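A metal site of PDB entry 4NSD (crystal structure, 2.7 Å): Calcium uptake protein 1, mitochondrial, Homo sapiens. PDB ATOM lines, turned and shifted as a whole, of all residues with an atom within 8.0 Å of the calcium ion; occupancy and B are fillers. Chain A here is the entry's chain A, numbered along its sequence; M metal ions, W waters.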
ATOM      1  N   PHE A 134     -10.606  17.788  -0.202  1.00  0.00           N
ATOM      2  CA  PHE A 134     -11.768  17.297   0.541  1.00  0.00           C
ATOM      3  C   PHE A 134     -12.584  16.393  -0.356  1.00  0.00           C
ATOM      4  O   PHE A 134     -13.055  15.339   0.054  1.00  0.00           O
ATOM      5  CB  PHE A 134     -12.622  18.472   1.016  1.00  0.00           C
ATOM      6  CG  PHE A 134     -13.783  18.053   1.889  1.00  0.00           C
ATOM      7  CD1 PHE A 134     -13.696  18.133   3.270  1.00  0.00           C
ATOM      8  CD2 PHE A 134     -14.936  17.558   1.324  1.00  0.00           C
ATOM      9  CE1 PHE A 134     -14.734  17.744   4.062  1.00  0.00           C
ATOM     10  CE2 PHE A 134     -15.986  17.156   2.117  1.00  0.00           C
ATOM     11  CZ  PHE A 134     -15.885  17.254   3.489  1.00  0.00           C
ATOM     12  N   LYS A 135     -12.781  16.844  -1.593  1.00  0.00           N
ATOM     13  CA  LYS A 135     -13.432  16.068  -2.632  1.00  0.00           C
ATOM     14  C   LYS A 135     -12.842  14.665  -2.693  1.00  0.00           C
ATOM     15  O   LYS A 135     -13.524  13.686  -2.414  1.00  0.00           O
ATOM     16  CB  LYS A 135     -13.201  16.736  -3.991  1.00  0.00           C
ATOM     17  CG  LYS A 135     -14.381  17.496  -4.554  1.00  0.00           C
ATOM     18  CD  LYS A 135     -13.964  18.194  -5.856  1.00  0.00           C
ATOM     19  CE  LYS A 135     -15.170  18.551  -6.738  1.00  0.00           C
ATOM     20  NZ  LYS A 135     -15.871  17.365  -7.344  1.00  0.00           N
ATOM     21  N   PHE A 137     -11.013  12.996  -0.873  1.00  0.00           N
ATOM     22  CA  PHE A 137     -11.125  12.248   0.372  1.00  0.00           C
ATOM     23  C   PHE A 137     -12.554  11.764   0.634  1.00  0.00           C
ATOM     24  O   PHE A 137     -12.760  10.611   1.008  1.00  0.00           O
ATOM     25  CB  PHE A 137     -10.604  13.061   1.555  1.00  0.00           C
ATOM     26  CG  PHE A 137      -9.137  12.864   1.810  1.00  0.00           C
ATOM     27  CD1 PHE A 137      -8.204  13.715   1.253  1.00  0.00           C
ATOM     28  CD2 PHE A 137      -8.700  11.816   2.595  1.00  0.00           C
ATOM     29  CE1 PHE A 137      -6.864  13.531   1.481  1.00  0.00           C
ATOM     30  CE2 PHE A 137      -7.352  11.617   2.828  1.00  0.00           C
ATOM     31  CZ  PHE A 137      -6.429  12.478   2.274  1.00  0.00           C
ATOM     32  N   ASP A 138     -13.516  12.635   0.454  1.00  0.00           N
ATOM     33  CA  ASP A 138     -14.918  12.281   0.600  1.00  0.00           C
ATOM     34  C   ASP A 138     -15.305  11.215  -0.414  1.00  0.00           C
ATOM     35  O   ASP A 138     -15.782  11.526  -1.512  1.00  0.00           O
ATOM     36  CB  ASP A 138     -15.773  13.531   0.383  1.00  0.00           C
ATOM     37  CG  ASP A 138     -17.245  13.257   0.511  1.00  0.00           C
ATOM     38  OD1 ASP A 138     -17.594  12.225   1.139  1.00  0.00           O
ATOM     39  OD2 ASP A 138     -18.036  14.077  -0.017  1.00  0.00           O
ATOM     40  N   LEU A 139     -15.113   9.953  -0.036  1.00  0.00           N
ATOM     41  CA  LEU A 139     -15.246   8.831  -0.967  1.00  0.00           C
ATOM     42  C   LEU A 139     -16.681   8.531  -1.366  1.00  0.00           C
ATOM     43  O   LEU A 139     -16.972   8.294  -2.538  1.00  0.00           O
ATOM     44  CB  LEU A 139     -14.600   7.581  -0.396  1.00  0.00           C
ATOM     45  CG  LEU A 139     -13.073   7.562  -0.486  1.00  0.00           C
ATOM     46  CD1 LEU A 139     -12.473   6.694   0.589  1.00  0.00           C
ATOM     47  CD2 LEU A 139     -12.634   7.098  -1.866  1.00  0.00           C
ATOM     48  N   ASN A 140     -17.581   8.547  -0.404  1.00  0.00           N
ATOM     49  CA  ASN A 140     -18.967   8.294  -0.724  1.00  0.00           C
ATOM     50  C   ASN A 140     -19.653   9.594  -1.130  1.00  0.00           C
ATOM     51  O   ASN A 140     -20.867   9.627  -1.296  1.00  0.00           O
ATOM     52  CB  ASN A 140     -19.691   7.651   0.455  1.00  0.00           C
ATOM     53  CG  ASN A 140     -19.598   8.502   1.690  1.00  0.00           C
ATOM     54  OD1 ASN A 140     -19.178   9.662   1.621  1.00  0.00           O
ATOM     55  ND2 ASN A 140     -20.007   7.943   2.826  1.00  0.00           N
ATOM     56  N   GLY A 141     -18.867  10.651  -1.283  1.00  0.00           N
ATOM     57  CA  GLY A 141     -19.403  11.958  -1.618  1.00  0.00           C
ATOM     58  C   GLY A 141     -20.567  12.402  -0.752  1.00  0.00           C
ATOM     59  O   GLY A 141     -21.499  13.057  -1.228  1.00  0.00           O
ATOM     60  N   ASP A 142     -20.536  12.053   0.540  1.00  0.00           N
ATOM     61  CA  ASP A 142     -21.655  12.361   1.418  1.00  0.00           C
ATOM     62  C   ASP A 142     -21.470  13.696   2.157  1.00  0.00           C
ATOM     63  O   ASP A 142     -21.993  13.871   3.261  1.00  0.00           O
ATOM     64  CB  ASP A 142     -21.868  11.239   2.426  1.00  0.00           C
ATOM     65  CG  ASP A 142     -20.812  11.265   3.519  1.00  0.00           C
ATOM     66  OD1 ASP A 142     -19.822  11.996   3.314  1.00  0.00           O
ATOM     67  OD2 ASP A 142     -20.977  10.583   4.560  1.00  0.00           O
ATOM     68  N   GLY A 143     -20.716  14.616   1.558  1.00  0.00           N
ATOM     69  CA  GLY A 143     -20.468  15.936   2.136  1.00  0.00           C
ATOM     70  C   GLY A 143     -19.589  15.965   3.387  1.00  0.00           C
ATOM     71  O   GLY A 143     -19.178  17.030   3.851  1.00  0.00           O
ATOM     72  N   GLU A 144     -19.321  14.796   3.942  1.00  0.00           N
ATOM     73  CA  GLU A 144     -18.459  14.686   5.113  1.00  0.00           C
ATOM     74  C   GLU A 144     -17.189  13.946   4.770  1.00  0.00           C
ATOM     75  O   GLU A 144     -16.968  13.561   3.633  1.00  0.00           O
ATOM     76  CB  GLU A 144     -19.171  13.915   6.216  1.00  0.00           C
ATOM     77  CG  GLU A 144     -20.267  14.694   6.923  1.00  0.00           C
ATOM     78  CD  GLU A 144     -20.873  13.898   8.051  1.00  0.00           C
ATOM     79  OE1 GLU A 144     -20.932  12.657   7.926  1.00  0.00           O
ATOM     80  OE2 GLU A 144     -21.283  14.505   9.068  1.00  0.00           O
ATOM     81  N   VAL A 145     -16.338  13.786   5.774  1.00  0.00           N
ATOM     82  CA  VAL A 145     -15.112  13.004   5.670  1.00  0.00           C
ATOM     83  C   VAL A 145     -14.790  12.439   7.040  1.00  0.00           C
ATOM     84  O   VAL A 145     -14.805  13.168   8.048  1.00  0.00           O
ATOM     85  CB  VAL A 145     -13.920  13.861   5.250  1.00  0.00           C
ATOM     86  CG1 VAL A 145     -12.648  13.041   5.400  1.00  0.00           C
ATOM     87  CG2 VAL A 145     -14.092  14.387   3.836  1.00  0.00           C
ATOM     88  N   ASP A 146     -14.500  11.140   7.083  1.00  0.00           N
ATOM     89  CA  ASP A 146     -14.325  10.451   8.359  1.00  0.00           C
ATOM     90  C   ASP A 146     -12.981   9.721   8.501  1.00  0.00           C
ATOM     91  O   ASP A 146     -12.111   9.793   7.623  1.00  0.00           O
ATOM     92  CB  ASP A 146     -15.480   9.483   8.599  1.00  0.00           C
ATOM     93  CG  ASP A 146     -15.804   8.617   7.377  1.00  0.00           C
ATOM     94  OD1 ASP A 146     -14.967   7.773   6.994  1.00  0.00           O
ATOM     95  OD2 ASP A 146     -16.899   8.794   6.812  1.00  0.00           O
ATOM     96  N   GLU A 149     -12.669   6.666   5.941  1.00  0.00           N
ATOM     97  CA  GLU A 149     -12.319   7.172   4.622  1.00  0.00           C
ATOM     98  C   GLU A 149     -10.878   7.651   4.541  1.00  0.00           C
ATOM     99  O   GLU A 149     -10.140   7.269   3.633  1.00  0.00           O
ATOM    100  CB  GLU A 149     -13.258   8.295   4.206  1.00  0.00           C
ATOM    101  CG  GLU A 149     -14.333   7.847   3.244  1.00  0.00           C
ATOM    102  CD  GLU A 149     -15.496   8.790   3.224  1.00  0.00           C
ATOM    103  OE1 GLU A 149     -15.484   9.725   4.053  1.00  0.00           O
ATOM    104  OE2 GLU A 149     -16.409   8.595   2.392  1.00  0.00           O
ATOM    105  N   PHE A 150     -10.477   8.502   5.485  1.00  0.00           N
ATOM    106  CA  PHE A 150      -9.073   8.885   5.539  1.00  0.00           C
ATOM    107  C   PHE A 150      -8.250   7.609   5.550  1.00  0.00           C
ATOM    108  O   PHE A 150      -7.293   7.452   4.782  1.00  0.00           O
ATOM    109  CB  PHE A 150      -8.766   9.727   6.779  1.00  0.00           C
ATOM    110  CG  PHE A 150      -7.360  10.262   6.796  1.00  0.00           C
ATOM    111  CD1 PHE A 150      -7.126  11.617   6.726  1.00  0.00           C
ATOM    112  CD2 PHE A 150      -6.279   9.398   6.856  1.00  0.00           C
ATOM    113  CE1 PHE A 150      -5.835  12.107   6.733  1.00  0.00           C
ATOM    114  CE2 PHE A 150      -4.988   9.881   6.857  1.00  0.00           C
ATOM    115  CZ  PHE A 150      -4.766  11.240   6.799  1.00  0.00           C
ATOM    116  N   LYS A 197     -16.330  13.972  12.066  1.00  0.00           N
ATOM    117  CA  LYS A 197     -16.537  14.150  10.644  1.00  0.00           C
ATOM    118  C   LYS A 197     -16.227  15.572  10.201  1.00  0.00           C
ATOM    119  O   LYS A 197     -16.776  16.532  10.734  1.00  0.00           O
ATOM    120  CB  LYS A 197     -17.964  13.758  10.262  1.00  0.00           C
ATOM    121  CG  LYS A 197     -18.221  12.257  10.319  1.00  0.00           C
ATOM    122  CD  LYS A 197     -19.699  11.940  10.309  1.00  0.00           C
ATOM    123  CE  LYS A 197     -20.421  12.611  11.474  1.00  0.00           C
ATOM    124  NZ  LYS A 197     -19.950  12.093  12.793  1.00  0.00           N
ATOM    125  N   LEU A 198     -15.360  15.671   9.205  1.00  0.00           N
ATOM    126  CA  LEU A 198     -14.789  16.928   8.754  1.00  0.00           C
ATOM    127  C   LEU A 198     -15.594  17.533   7.604  1.00  0.00           C
ATOM    128  O   LEU A 198     -15.946  16.849   6.657  1.00  0.00           O
ATOM    129  CB  LEU A 198     -13.352  16.666   8.294  1.00  0.00           C
ATOM    130  CG  LEU A 198     -12.315  17.762   8.089  1.00  0.00           C
ATOM    131  CD1 LEU A 198     -11.390  17.368   6.922  1.00  0.00           C
ATOM    132  CD2 LEU A 198     -12.949  19.121   7.856  1.00  0.00           C
HETATM  133 CA    CA M   1     -17.600  10.959   3.288  1.00  0.00          CA
HETATM  134  O   HOH W   1     -18.566   9.563   5.201  1.00  0.00           O
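Residues that only touch the calcium ion: Val 145 (3.97 Å).
The calcium ion is bound by OD1 of Asp 142 (2.5 Å), OD1 of Asp 138 (2.5 Å), water W1 (2.6 Å), OE1 of Glu 149 (2.6 Å), OD1 of Asn 140 (2.6 Å), O of Glu 144 (2.7 Å) and OE2 of Glu 149 (2.8 Å).
The calcium ion has seven donor atoms within binding distance.
Water W1 lies within hydrogen-bond range of OD2 of Asp 146 (2.4 Å), OD2 of Asp 142 (2.7 Å) and ND2 of Asn 140 (3.2 Å).
OD1 of Asp 138 lies close to N of Gly 141.
The backbone NH (N) of Gly 143 sits at hydrogen-bond distance from the side-chain carboxylate (OD2) of Asp 138.
N of Glu 149 sits at hydrogen-bond distance from OD1 of Asp 146 (2.8 Å).
OE2 of Glu 149 lies close to N of Leu 139 (3.1 Å).
The backbone NH (N) of Leu 198 is in hydrogen-bond range of the backbone carbonyl oxygen (O) of Val 145.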
